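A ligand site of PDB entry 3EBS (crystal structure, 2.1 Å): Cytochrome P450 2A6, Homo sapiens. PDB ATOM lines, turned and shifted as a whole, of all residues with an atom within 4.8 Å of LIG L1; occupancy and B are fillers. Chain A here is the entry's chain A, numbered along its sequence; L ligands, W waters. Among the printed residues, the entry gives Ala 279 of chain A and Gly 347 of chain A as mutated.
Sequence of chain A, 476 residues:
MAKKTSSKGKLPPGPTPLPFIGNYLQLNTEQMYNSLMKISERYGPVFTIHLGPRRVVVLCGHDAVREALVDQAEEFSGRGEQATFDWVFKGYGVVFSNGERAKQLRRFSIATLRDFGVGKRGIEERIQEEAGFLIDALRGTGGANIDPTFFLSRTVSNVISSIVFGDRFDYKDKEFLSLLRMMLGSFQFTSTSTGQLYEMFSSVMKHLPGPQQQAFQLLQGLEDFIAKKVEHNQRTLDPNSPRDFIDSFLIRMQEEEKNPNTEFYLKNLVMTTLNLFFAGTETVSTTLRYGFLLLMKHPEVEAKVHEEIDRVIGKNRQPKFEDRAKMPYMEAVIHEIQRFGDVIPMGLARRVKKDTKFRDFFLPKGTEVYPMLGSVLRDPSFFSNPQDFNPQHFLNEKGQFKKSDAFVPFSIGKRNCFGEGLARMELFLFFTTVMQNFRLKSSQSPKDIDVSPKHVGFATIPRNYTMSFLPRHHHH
An iron atom (FE1) of LIG L1 is bound by the side-chain sulfur (SG) of Cys 417.
An oxygen (O1) of LIG L1 is in hydrogen-bond range of the side-chain hydroxyl (OG) of Ser 411 (2.5 Å).
The backbone carbonyl oxygen (O) of Arg 415 sits close to an oxygen (O2) of LIG L1 (3.1 Å).
NE of Arg 415 lies within salt-bridge range of O3 of LIG L1 (2.7 Å).
NH2 of Arg 79 lies within salt-bridge range of O4 of LIG L1 (2.7 Å).
The guanidinium group (NE) of Arg 350 is in salt-bridge range of an oxygen (O2) of LIG L1 (2.8 Å).
NH1 of Arg 106 lies within salt-bridge range of O3 of LIG L1, at 2.9 Å.
The backbone NH (N) of Cys 417 is in hydrogen-bond range of the backbone carbonyl oxygen (O) of Phe 410 (3.1 Å).
The guanidinium group of Arg 415 lies within hydrogen-bond range of the backbone carbonyl oxygen of Val 95, 2.9 Å away.
O of Val 95 sits at hydrogen-bond distance from NE of Arg 79.
NH1 of Arg 79 is in hydrogen-bond range of O of Leu 348 (3.4 Å).
NH2 of Arg 350 is in hydrogen-bond range of O of Ile 412 (2.9 Å).
O of Asn 416 is in hydrogen-bond range of NH1 of Arg 106 (2.7 Å).
OG1 of Thr 283 sits at hydrogen-bond distance from O of Ala 279, at 3.1 Å.
The side-chain hydroxyl of Thr 287 lies within hydrogen-bond range of the backbone carbonyl oxygen of Thr 283 (2.9 Å).
O of Val 95 sits close to O4 of LIG L1 (3.5 Å).
O of Val 94 touches O4 of LIG L1, 3.8 Å away.
Leu 276 touches LIG L1.
Ala 279 touches LIG L1 (CB to C4, 3.3 Å).
Gly 280 touches LIG L1 (CA to C24, 3.6 Å).
Thr 283 touches LIG L1 (OG1 to C16, 3.1 Å).
CG2 of Val 284 touches C18 of LIG L1 (3.8 Å).
Thr 287 touches LIG L1.
NE2 of Gln 338 touches C19 of LIG L1, 3.5 Å away.
Leu 348 touches LIG L1.
Leu 373 touches LIG L1 (CD1 to C9, 3.8 Å).
O of Pro 409 touches C17 of LIG L1, at 3.5 Å.
Phe 410 touches LIG L1 (CE1 to C15, 3.5 Å).
CA of Asn 416 touches C11 of LIG L1 (3.8 Å).
CZ of Phe 418 touches C31 of LIG L1, 3.1 Å away.
CA of Gly 419 touches C22 of LIG L1 (3.5 Å).
Ala 423 touches LIG L1.
23 residues have an atom within 4 Å of LIG L1: Arg 79, Val 94, Val 95, Arg 106, Leu 276, Ala 279, Gly 280, Thr 283, Val 284, Thr 287, Gln 338, Leu 348, Arg 350, Leu 373, Pro 409, Phe 410, Ser 411, Arg 415, Asn 416, Cys 417, Phe 418, Gly 419 and Ala 423.
The nearest printed residue that does not touch LIG L1 is Ile 344 (4.1 Å).
Water W1 lies within hydrogen-bond range of an oxygen (O3) of LIG L1 (2.7 Å), the backbone carbonyl oxygen of Val 94 (3.0 Å) and the guanidinium group of Arg 415 (3.1 Å).
Water W2 lies within hydrogen-bond range of the backbone carbonyl oxygen of Leu 348, an oxygen (O1) of LIG L1 and the side-chain hydroxyl of Ser 411.
Water W3 bridges OG1 of Thr 287 and NE2 of Gln 338.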
ATOM      1  N   LEU A  69      -6.587   7.611  -5.963  1.00  0.00           N
ATOM      2  CA  LEU A  69      -6.404   6.216  -5.589  1.00  0.00           C
ATOM      3  C   LEU A  69      -7.697   5.446  -5.328  1.00  0.00           C
ATOM      4  O   LEU A  69      -7.724   4.238  -5.516  1.00  0.00           O
ATOM      5  CB  LEU A  69      -5.430   6.094  -4.388  1.00  0.00           C
ATOM      6  CG  LEU A  69      -3.942   5.814  -4.727  1.00  0.00           C
ATOM      7  CD1 LEU A  69      -3.336   6.928  -5.581  1.00  0.00           C
ATOM      8  CD2 LEU A  69      -3.080   5.526  -3.477  1.00  0.00           C
ATOM      9  N   ARG A  79       1.605  -0.459 -10.417  1.00  0.00           N
ATOM     10  CA  ARG A  79       2.648  -0.342  -9.448  1.00  0.00           C
ATOM     11  C   ARG A  79       3.826   0.357 -10.104  1.00  0.00           C
ATOM     12  O   ARG A  79       4.230  -0.020 -11.205  1.00  0.00           O
ATOM     13  CB  ARG A  79       3.044  -1.720  -8.930  1.00  0.00           C
ATOM     14  CG  ARG A  79       4.384  -1.796  -8.138  1.00  0.00           C
ATOM     15  CD  ARG A  79       4.348  -1.129  -6.774  1.00  0.00           C
ATOM     16  NE  ARG A  79       3.446  -1.801  -5.828  1.00  0.00           N
ATOM     17  CZ  ARG A  79       2.469  -1.199  -5.138  1.00  0.00           C
ATOM     18  NH1 ARG A  79       2.272   0.103  -5.288  1.00  0.00           N
ATOM     19  NH2 ARG A  79       1.703  -1.883  -4.292  1.00  0.00           N
ATOM     20  N   VAL A  94       4.723 -10.541  -5.718  1.00  0.00           N
ATOM     21  CA  VAL A  94       3.386  -9.906  -5.635  1.00  0.00           C
ATOM     22  C   VAL A  94       3.388  -8.366  -5.504  1.00  0.00           C
ATOM     23  O   VAL A  94       2.496  -7.708  -6.055  1.00  0.00           O
ATOM     24  CB  VAL A  94       2.526 -10.583  -4.519  1.00  0.00           C
ATOM     25  CG1 VAL A  94       3.159 -10.360  -3.109  1.00  0.00           C
ATOM     26  CG2 VAL A  94       1.077 -10.141  -4.591  1.00  0.00           C
ATOM     27  N   VAL A  95       4.380  -7.824  -4.790  1.00  0.00           N
ATOM     28  CA  VAL A  95       4.435  -6.382  -4.438  1.00  0.00           C
ATOM     29  C   VAL A  95       4.877  -5.465  -5.599  1.00  0.00           C
ATOM     30  O   VAL A  95       4.205  -4.484  -5.918  1.00  0.00           O
ATOM     31  CB  VAL A  95       5.411  -6.089  -3.217  1.00  0.00           C
ATOM     32  CG1 VAL A  95       5.599  -4.598  -3.054  1.00  0.00           C
ATOM     33  CG2 VAL A  95       4.921  -6.687  -1.932  1.00  0.00           C
ATOM     34  N   ARG A 106      -1.575 -11.568  -6.322  1.00  0.00           N
ATOM     35  CA  ARG A 106      -2.423 -10.956  -5.291  1.00  0.00           C
ATOM     36  C   ARG A 106      -3.626 -11.832  -4.910  1.00  0.00           C
ATOM     37  O   ARG A 106      -3.919 -12.032  -3.720  1.00  0.00           O
ATOM     38  CB  ARG A 106      -2.859  -9.540  -5.640  1.00  0.00           C
ATOM     39  CG  ARG A 106      -3.511  -8.806  -4.471  1.00  0.00           C
ATOM     40  CD  ARG A 106      -3.681  -7.325  -4.750  1.00  0.00           C
ATOM     41  NE  ARG A 106      -4.686  -6.727  -3.877  1.00  0.00           N
ATOM     42  CZ  ARG A 106      -4.459  -5.739  -3.024  1.00  0.00           C
ATOM     43  NH1 ARG A 106      -3.241  -5.218  -2.910  1.00  0.00           N
ATOM     44  NH2 ARG A 106      -5.451  -5.276  -2.277  1.00  0.00           N
ATOM     45  N   LEU A 113      -3.256 -16.840   2.616  1.00  0.00           N
ATOM     46  CA  LEU A 113      -3.235 -16.290   3.968  1.00  0.00           C
ATOM     47  C   LEU A 113      -4.526 -16.603   4.777  1.00  0.00           C
ATOM     48  O   LEU A 113      -4.432 -16.889   5.995  1.00  0.00           O
ATOM     49  CB  LEU A 113      -2.985 -14.788   3.923  1.00  0.00           C
ATOM     50  CG  LEU A 113      -1.638 -14.072   4.164  1.00  0.00           C
ATOM     51  CD1 LEU A 113      -0.362 -14.933   4.153  1.00  0.00           C
ATOM     52  CD2 LEU A 113      -1.553 -12.956   3.143  1.00  0.00           C
ATOM     53  N   ILE A 160       4.153 -14.164  10.737  1.00  0.00           N
ATOM     54  CA  ILE A 160       4.198 -14.475   9.317  1.00  0.00           C
ATOM     55  C   ILE A 160       5.077 -15.714   8.976  1.00  0.00           C
ATOM     56  O   ILE A 160       4.760 -16.469   8.034  1.00  0.00           O
ATOM     57  CB  ILE A 160       4.533 -13.238   8.439  1.00  0.00           C
ATOM     58  CG1 ILE A 160       4.108 -13.498   6.984  1.00  0.00           C
ATOM     59  CG2 ILE A 160       6.054 -12.761   8.643  1.00  0.00           C
ATOM     60  CD1 ILE A 160       2.564 -13.390   6.724  1.00  0.00           C
ATOM     61  N   LEU A 276       6.124 -11.313   1.508  1.00  0.00           N
ATOM     62  CA  LEU A 276       5.337 -11.619   2.745  1.00  0.00           C
ATOM     63  C   LEU A 276       6.170 -11.687   4.046  1.00  0.00           C
ATOM     64  O   LEU A 276       5.792 -11.130   5.070  1.00  0.00           O
ATOM     65  CB  LEU A 276       4.489 -12.908   2.560  1.00  0.00           C
ATOM     66  CG  LEU A 276       3.354 -12.923   1.491  1.00  0.00           C
ATOM     67  CD1 LEU A 276       2.628 -14.286   1.324  1.00  0.00           C
ATOM     68  CD2 LEU A 276       2.362 -11.770   1.693  1.00  0.00           C
ATOM     69  N   ALA A 279       7.376  -7.907   4.434  1.00  0.00           N
ATOM     70  CA  ALA A 279       6.282  -6.953   4.699  1.00  0.00           C
ATOM     71  C   ALA A 279       5.624  -7.259   6.045  1.00  0.00           C
ATOM     72  O   ALA A 279       5.253  -6.359   6.792  1.00  0.00           O
ATOM     73  CB  ALA A 279       5.217  -6.952   3.528  1.00  0.00           C
ATOM     74  N   GLY A 280       5.540  -8.562   6.336  1.00  0.00           N
ATOM     75  CA  GLY A 280       4.888  -9.058   7.533  1.00  0.00           C
ATOM     76  C   GLY A 280       5.717  -8.942   8.785  1.00  0.00           C
ATOM     77  O   GLY A 280       5.184  -9.166   9.867  1.00  0.00           O
ATOM     78  N   THR A 283       7.425  -3.546   8.970  1.00  0.00           N
ATOM     79  CA  THR A 283       6.541  -2.394   9.185  1.00  0.00           C
ATOM     80  C   THR A 283       5.891  -2.431  10.579  1.00  0.00           C
ATOM     81  O   THR A 283       5.943  -1.425  11.300  1.00  0.00           O
ATOM     82  CB  THR A 283       5.453  -2.248   8.069  1.00  0.00           C
ATOM     83  OG1 THR A 283       4.783  -3.500   7.905  1.00  0.00           O
ATOM     84  CG2 THR A 283       6.097  -1.884   6.735  1.00  0.00           C
ATOM     85  N   VAL A 284       5.350  -3.593  10.972  1.00  0.00           N
ATOM     86  CA  VAL A 284       4.787  -3.770  12.310  1.00  0.00           C
ATOM     87  C   VAL A 284       5.843  -3.562  13.406  1.00  0.00           C
ATOM     88  O   VAL A 284       5.603  -2.866  14.409  1.00  0.00           O
ATOM     89  CB  VAL A 284       4.042  -5.144  12.501  1.00  0.00           C
ATOM     90  CG1 VAL A 284       3.576  -5.339  13.972  1.00  0.00           C
ATOM     91  CG2 VAL A 284       2.853  -5.278  11.531  1.00  0.00           C
ATOM     92  N   THR A 287       6.611   0.009  13.864  1.00  0.00           N
ATOM     93  CA  THR A 287       5.447   0.622  14.492  1.00  0.00           C
ATOM     94  C   THR A 287       5.457   0.352  16.015  1.00  0.00           C
ATOM     95  O   THR A 287       5.178   1.254  16.783  1.00  0.00           O
ATOM     96  CB  THR A 287       4.100   0.153  13.825  1.00  0.00           C
ATOM     97  OG1 THR A 287       4.107   0.450  12.426  1.00  0.00           O
ATOM     98  CG2 THR A 287       2.875   0.788  14.493  1.00  0.00           C
ATOM     99  N   GLN A 338       0.273   4.838  14.565  1.00  0.00           N
ATOM    100  CA  GLN A 338       0.359   4.690  13.128  1.00  0.00           C
ATOM    101  C   GLN A 338       0.312   6.066  12.413  1.00  0.00           C
ATOM    102  O   GLN A 338       0.997   6.271  11.419  1.00  0.00           O
ATOM    103  CB  GLN A 338      -0.745   3.756  12.604  1.00  0.00           C
ATOM    104  CG  GLN A 338      -0.721   2.321  13.125  1.00  0.00           C
ATOM    105  CD  GLN A 338      -1.529   1.377  12.210  1.00  0.00           C
ATOM    106  OE1 GLN A 338      -2.724   1.119  12.433  1.00  0.00           O
ATOM    107  NE2 GLN A 338      -0.868   0.851  11.188  1.00  0.00           N
ATOM    108  N   ILE A 344       5.416   4.567   6.197  1.00  0.00           N
ATOM    109  CA  ILE A 344       5.635   4.674   4.756  1.00  0.00           C
ATOM    110  C   ILE A 344       5.109   6.038   4.311  1.00  0.00           C
ATOM    111  O   ILE A 344       3.951   6.156   3.812  1.00  0.00           O
ATOM    112  CB  ILE A 344       4.974   3.489   3.987  1.00  0.00           C
ATOM    113  CG1 ILE A 344       5.142   2.183   4.776  1.00  0.00           C
ATOM    114  CG2 ILE A 344       5.498   3.394   2.546  1.00  0.00           C
ATOM    115  CD1 ILE A 344       6.518   1.568   4.733  1.00  0.00           C
ATOM    116  N   GLY A 347       4.175   6.589   0.481  1.00  0.00           N
ATOM    117  CA  GLY A 347       3.573   5.374  -0.008  1.00  0.00           C
ATOM    118  C   GLY A 347       4.502   4.375  -0.688  1.00  0.00           C
ATOM    119  O   GLY A 347       5.742   4.364  -0.505  1.00  0.00           O
ATOM    120  N   LEU A 348       3.879   3.493  -1.460  1.00  0.00           N
ATOM    121  CA  LEU A 348       4.650   2.743  -2.400  1.00  0.00           C
ATOM    122  C   LEU A 348       4.174   3.186  -3.782  1.00  0.00           C
ATOM    123  O   LEU A 348       2.954   3.224  -4.059  1.00  0.00           O
ATOM    124  CB  LEU A 348       4.619   1.241  -2.110  1.00  0.00           C
ATOM    125  CG  LEU A 348       5.456   0.240  -2.916  1.00  0.00           C
ATOM    126  CD1 LEU A 348       6.973   0.315  -2.750  1.00  0.00           C
ATOM    127  CD2 LEU A 348       4.954  -1.193  -2.637  1.00  0.00           C
ATOM    128  N   ARG A 350       2.846   4.052  -7.199  1.00  0.00           N
ATOM    129  CA  ARG A 350       1.879   3.543  -8.140  1.00  0.00           C
ATOM    130  C   ARG A 350       2.282   4.040  -9.545  1.00  0.00           C
ATOM    131  O   ARG A 350       3.337   4.691  -9.709  1.00  0.00           O
ATOM    132  CB  ARG A 350       0.475   4.054  -7.733  1.00  0.00           C
ATOM    133  CG  ARG A 350       0.026   3.683  -6.283  1.00  0.00           C
ATOM    134  CD  ARG A 350      -0.245   2.170  -6.223  1.00  0.00           C
ATOM    135  NE  ARG A 350      -1.144   1.739  -5.155  1.00  0.00           N
ATOM    136  CZ  ARG A 350      -2.462   1.900  -5.145  1.00  0.00           C
ATOM    137  NH1 ARG A 350      -3.060   2.505  -6.149  1.00  0.00           N
ATOM    138  NH2 ARG A 350      -3.185   1.466  -4.128  1.00  0.00           N
ATOM    139  N   LEU A 373       1.413   9.614   1.515  1.00  0.00           N
ATOM    140  CA  LEU A 373       0.587   9.159   2.639  1.00  0.00           C
ATOM    141  C   LEU A 373       0.814   9.983   3.877  1.00  0.00           C
ATOM    142  O   LEU A 373      -0.121  10.206   4.624  1.00  0.00           O
ATOM    143  CB  LEU A 373       0.869   7.706   2.959  1.00  0.00           C
ATOM    144  CG  LEU A 373       0.620   6.745   1.809  1.00  0.00           C
ATOM    145  CD1 LEU A 373       0.941   5.354   2.294  1.00  0.00           C
ATOM    146  CD2 LEU A 373      -0.837   6.864   1.283  1.00  0.00           C
ATOM    147  N   PRO A 409      -2.523   4.710   6.745  1.00  0.00           N
ATOM    148  CA  PRO A 409      -1.182   4.109   6.837  1.00  0.00           C
ATOM    149  C   PRO A 409      -0.990   2.845   5.989  1.00  0.00           C
ATOM    150  O   PRO A 409       0.136   2.545   5.599  1.00  0.00           O
ATOM    151  CB  PRO A 409      -1.035   3.782   8.331  1.00  0.00           C
ATOM    152  CG  PRO A 409      -2.335   3.703   8.876  1.00  0.00           C
ATOM    153  CD  PRO A 409      -3.252   4.575   8.022  1.00  0.00           C
ATOM    154  N   PHE A 410      -2.076   2.139   5.690  1.00  0.00           N
ATOM    155  CA  PHE A 410      -2.028   0.983   4.768  1.00  0.00           C
ATOM    156  C   PHE A 410      -2.366   1.370   3.296  1.00  0.00           C
ATOM    157  O   PHE A 410      -2.585   0.490   2.419  1.00  0.00           O
ATOM    158  CB  PHE A 410      -2.930  -0.134   5.282  1.00  0.00           C
ATOM    159  CG  PHE A 410      -2.723  -0.505   6.731  1.00  0.00           C
ATOM    160  CD1 PHE A 410      -1.712  -1.375   7.099  1.00  0.00           C
ATOM    161  CD2 PHE A 410      -3.588  -0.005   7.732  1.00  0.00           C
ATOM    162  CE1 PHE A 410      -1.521  -1.733   8.446  1.00  0.00           C
ATOM    163  CE2 PHE A 410      -3.420  -0.360   9.077  1.00  0.00           C
ATOM    164  CZ  PHE A 410      -2.390  -1.243   9.434  1.00  0.00           C
ATOM    165  N   SER A 411      -2.412   2.678   3.042  1.00  0.00           N
ATOM    166  CA  SER A 411      -2.811   3.214   1.744  1.00  0.00           C
ATOM    167  C   SER A 411      -4.293   2.839   1.436  1.00  0.00           C
ATOM    168  O   SER A 411      -5.030   2.330   2.297  1.00  0.00           O
ATOM    169  CB  SER A 411      -1.846   2.745   0.629  1.00  0.00           C
ATOM    170  OG  SER A 411      -2.076   3.408  -0.616  1.00  0.00           O
ATOM    171  N   ILE A 412      -4.712   3.101   0.203  1.00  0.00           N
ATOM    172  CA  ILE A 412      -6.099   2.872  -0.193  1.00  0.00           C
ATOM    173  C   ILE A 412      -6.136   2.493  -1.670  1.00  0.00           C
ATOM    174  O   ILE A 412      -5.148   2.647  -2.370  1.00  0.00           O
ATOM    175  CB  ILE A 412      -7.007   4.117   0.115  1.00  0.00           C
ATOM    176  CG1 ILE A 412      -6.242   5.432  -0.067  1.00  0.00           C
ATOM    177  CG2 ILE A 412      -7.527   4.043   1.526  1.00  0.00           C
ATOM    178  CD1 ILE A 412      -7.098   6.669  -0.232  1.00  0.00           C
ATOM    179  N   ARG A 415      -4.385  -1.504  -5.042  1.00  0.00           N
ATOM    180  CA  ARG A 415      -3.127  -2.125  -4.685  1.00  0.00           C
ATOM    181  C   ARG A 415      -2.727  -1.765  -3.239  1.00  0.00           C
ATOM    182  O   ARG A 415      -1.547  -1.766  -2.895  1.00  0.00           O
ATOM    183  CB  ARG A 415      -2.009  -1.721  -5.660  1.00  0.00           C
ATOM    184  CG  ARG A 415      -2.126  -2.174  -7.093  1.00  0.00           C
ATOM    185  CD  ARG A 415      -1.914  -3.688  -7.347  1.00  0.00           C
ATOM    186  NE  ARG A 415      -0.611  -4.204  -6.927  1.00  0.00           N
ATOM    187  CZ  ARG A 415       0.476  -4.324  -7.703  1.00  0.00           C
ATOM    188  NH1 ARG A 415       1.612  -4.796  -7.190  1.00  0.00           N
ATOM    189  NH2 ARG A 415       0.432  -3.963  -8.979  1.00  0.00           N
ATOM    190  N   ASN A 416      -3.739  -1.485  -2.383  1.00  0.00           N
ATOM    191  CA  ASN A 416      -3.538  -1.283  -0.949  1.00  0.00           C
ATOM    192  C   ASN A 416      -2.990  -2.496  -0.215  1.00  0.00           C
ATOM    193  O   ASN A 416      -2.998  -3.621  -0.732  1.00  0.00           O
ATOM    194  CB  ASN A 416      -4.818  -0.776  -0.258  1.00  0.00           C
ATOM    195  CG  ASN A 416      -5.949  -1.835  -0.193  1.00  0.00           C
ATOM    196  OD1 ASN A 416      -5.939  -2.838  -0.906  1.00  0.00           O
ATOM    197  ND2 ASN A 416      -6.926  -1.599   0.677  1.00  0.00           N
ATOM    198  N   CYS A 417      -2.516  -2.258   1.003  1.00  0.00           N
ATOM    199  CA  CYS A 417      -1.952  -3.306   1.831  1.00  0.00           C
ATOM    200  C   CYS A 417      -2.958  -4.462   2.095  1.00  0.00           C
ATOM    201  O   CYS A 417      -3.938  -4.244   2.711  1.00  0.00           O
ATOM    202  CB  CYS A 417      -1.497  -2.715   3.175  1.00  0.00           C
ATOM    203  SG  CYS A 417      -0.904  -3.953   4.251  1.00  0.00           S
ATOM    204  N   PHE A 418      -2.651  -5.693   1.664  1.00  0.00           N
ATOM    205  CA  PHE A 418      -3.539  -6.823   1.990  1.00  0.00           C
ATOM    206  C   PHE A 418      -3.167  -7.564   3.265  1.00  0.00           C
ATOM    207  O   PHE A 418      -3.880  -8.464   3.690  1.00  0.00           O
ATOM    208  CB  PHE A 418      -3.856  -7.764   0.816  1.00  0.00           C
ATOM    209  CG  PHE A 418      -2.664  -8.470   0.220  1.00  0.00           C
ATOM    210  CD1 PHE A 418      -2.054  -9.543   0.882  1.00  0.00           C
ATOM    211  CD2 PHE A 418      -2.190  -8.105  -1.032  1.00  0.00           C
ATOM    212  CE1 PHE A 418      -0.966 -10.223   0.321  1.00  0.00           C
ATOM    213  CE2 PHE A 418      -1.098  -8.791  -1.604  1.00  0.00           C
ATOM    214  CZ  PHE A 418      -0.478  -9.842  -0.925  1.00  0.00           C
ATOM    215  N   GLY A 419      -2.060  -7.120   3.876  1.00  0.00           N
ATOM    216  CA  GLY A 419      -1.686  -7.515   5.246  1.00  0.00           C
ATOM    217  C   GLY A 419      -2.323  -6.662   6.342  1.00  0.00           C
ATOM    218  O   GLY A 419      -2.109  -6.920   7.508  1.00  0.00           O
ATOM    219  N   LEU A 422      -4.127  -8.600   9.415  1.00  0.00           N
ATOM    220  CA  LEU A 422      -3.060  -9.218  10.195  1.00  0.00           C
ATOM    221  C   LEU A 422      -2.317  -8.162  11.015  1.00  0.00           C
ATOM    222  O   LEU A 422      -2.246  -8.268  12.222  1.00  0.00           O
ATOM    223  CB  LEU A 422      -2.097  -9.989   9.264  1.00  0.00           C
ATOM    224  CG  LEU A 422      -0.930 -10.679  10.007  1.00  0.00           C
ATOM    225  CD1 LEU A 422      -1.433 -11.749  10.967  1.00  0.00           C
ATOM    226  CD2 LEU A 422       0.093 -11.222   9.057  1.00  0.00           C
ATOM    227  N   ALA A 423      -1.823  -7.120  10.348  1.00  0.00           N
ATOM    228  CA  ALA A 423      -1.141  -5.981  11.004  1.00  0.00           C
ATOM    229  C   ALA A 423      -1.964  -5.396  12.166  1.00  0.00           C
ATOM    230  O   ALA A 423      -1.441  -5.280  13.267  1.00  0.00           O
ATOM    231  CB  ALA A 423      -0.736  -4.910   9.991  1.00  0.00           C
ATOM    232  N   LEU A 427      -0.785  -5.496  16.138  1.00  0.00           N
ATOM    233  CA  LEU A 427      -0.606  -4.253  16.872  1.00  0.00           C
ATOM    234  C   LEU A 427      -1.491  -4.181  18.107  1.00  0.00           C
ATOM    235  O   LEU A 427      -1.015  -3.783  19.188  1.00  0.00           O
ATOM    236  CB  LEU A 427      -0.885  -3.047  15.962  1.00  0.00           C
ATOM    237  CG  LEU A 427       0.078  -2.686  14.822  1.00  0.00           C
ATOM    238  CD1 LEU A 427      -0.448  -1.420  14.145  1.00  0.00           C
ATOM    239  CD2 LEU A 427       1.530  -2.497  15.341  1.00  0.00           C
HETATM  240  C1  LIG L   1       1.465  -2.948   0.447  1.00  0.00           C
HETATM  241  C2  LIG L   1       1.830  -0.508   4.612  1.00  0.00           C
HETATM  242  C3  LIG L   1       1.819  -4.554   7.213  1.00  0.00           C
HETATM  243  C4  LIG L   1       1.946  -7.068   3.019  1.00  0.00           C
HETATM  244  C5  LIG L   1       1.555  -1.954   1.368  1.00  0.00           C
HETATM  245  C6  LIG L   1       1.579  -0.558   1.041  1.00  0.00           C
HETATM  246  C7  LIG L   1       1.675   0.119   2.184  1.00  0.00           C
HETATM  247  C8  LIG L   1       1.701  -0.843   3.278  1.00  0.00           C
HETATM  248  C9  LIG L   1       1.709   1.682   2.325  1.00  0.00           C
HETATM  249  C10 LIG L   1       1.470   0.055  -0.368  1.00  0.00           C
HETATM  250  C11 LIG L   1       0.059  -0.182  -0.945  1.00  0.00           C
HETATM  251  C12 LIG L   1      -0.212   0.707  -2.139  1.00  0.00           C
HETATM  252  O1  LIG L   1      -1.105   1.553  -2.011  1.00  0.00           O
HETATM  253  O2  LIG L   1       0.447   0.583  -3.198  1.00  0.00           O
HETATM  254  C13 LIG L   1       1.870  -1.366   5.712  1.00  0.00           C
HETATM  255  C14 LIG L   1       1.923  -0.989   7.119  1.00  0.00           C
HETATM  256  C15 LIG L   1       1.907  -2.117   7.845  1.00  0.00           C
HETATM  257  C16 LIG L   1       1.833  -3.235   6.917  1.00  0.00           C
HETATM  258  C17 LIG L   1       1.998   0.454   7.681  1.00  0.00           C
HETATM  259  C18 LIG L   1       1.965  -2.274   9.401  1.00  0.00           C
HETATM  260  C19 LIG L   1       1.673  -1.310  10.277  1.00  0.00           C
HETATM  261  C20 LIG L   1       1.827  -5.570   6.278  1.00  0.00           C
HETATM  262  C21 LIG L   1       1.764  -6.984   6.617  1.00  0.00           C
HETATM  263  C22 LIG L   1       1.763  -7.691   5.488  1.00  0.00           C
HETATM  264  C23 LIG L   1       1.873  -6.754   4.363  1.00  0.00           C
HETATM  265  C24 LIG L   1       1.640  -7.567   8.045  1.00  0.00           C
HETATM  266  C25 LIG L   1       1.717  -9.257   5.511  1.00  0.00           C
HETATM  267  C26 LIG L   1       1.097  -9.996   4.577  1.00  0.00           C
HETATM  268  C27 LIG L   1       1.822  -6.227   1.935  1.00  0.00           C
HETATM  269  C28 LIG L   1       1.815  -6.620   0.540  1.00  0.00           C
HETATM  270  C29 LIG L   1       1.629  -5.321  -0.252  1.00  0.00           C
HETATM  271  C30 LIG L   1       1.591  -4.282   0.726  1.00  0.00           C
HETATM  272  C31 LIG L   1       1.945  -8.088  -0.013  1.00  0.00           C
HETATM  273  C32 LIG L   1       1.540  -5.127  -1.782  1.00  0.00           C
HETATM  274  C33 LIG L   1       0.121  -5.400  -2.307  1.00  0.00           C
HETATM  275  C34 LIG L   1       0.123  -5.120  -3.804  1.00  0.00           C
HETATM  276  O3  LIG L   1      -0.870  -5.432  -4.513  1.00  0.00           O
HETATM  277  O4  LIG L   1       1.127  -4.567  -4.310  1.00  0.00           O
HETATM  278  N1  LIG L   1       1.622  -2.114   2.737  1.00  0.00           N
HETATM  279  N2  LIG L   1       1.788  -2.750   5.631  1.00  0.00           N
HETATM  280  N3  LIG L   1       1.890  -5.447   4.875  1.00  0.00           N
HETATM  281  N4  LIG L   1       1.701  -4.847   2.000  1.00  0.00           N
HETATM  282 FE1  LIG L   1       1.573  -3.765   3.870  1.00  0.00          FE
HETATM  283  O1  LG2 L   2       9.154  -6.950   0.171  1.00  0.00           O
HETATM  284  C1  LG2 L   2      10.157  -6.362   0.555  1.00  0.00           C
HETATM  285  C2  LG2 L   2      11.528  -6.925   0.349  1.00  0.00           C
HETATM  286  N1  LG2 L   2      10.133  -5.181   1.176  1.00  0.00           N
HETATM  287  C3  LG2 L   2       9.029  -4.462   1.495  1.00  0.00           C
HETATM  288  C4  LG2 L   2       9.246  -3.255   2.162  1.00  0.00           C
HETATM  289  C5  LG2 L   2       8.158  -2.460   2.524  1.00  0.00           C
HETATM  290  C6  LG2 L   2       6.860  -2.856   2.212  1.00  0.00           C
HETATM  291  C7  LG2 L   2       6.632  -4.068   1.552  1.00  0.00           C
HETATM  292  C8  LG2 L   2       7.723  -4.873   1.189  1.00  0.00           C
HETATM  293  O2  LG2 L   2       5.816  -2.046   2.593  1.00  0.00           O
HETATM  294  C9  LG2 L   2       4.869  -1.604   1.619  1.00  0.00           C
HETATM  295  C10 LG2 L   2       5.261  -0.239   1.112  1.00  0.00           C
HETATM  296  O   HOH W   1      -0.496  -7.280  -6.385  1.00  0.00           O
HETATM  297  O   HOH W   2       0.899   3.904  -1.959  1.00  0.00           O
HETATM  298  O   HOH W   3       1.958   1.844  11.215  1.00  0.00           O
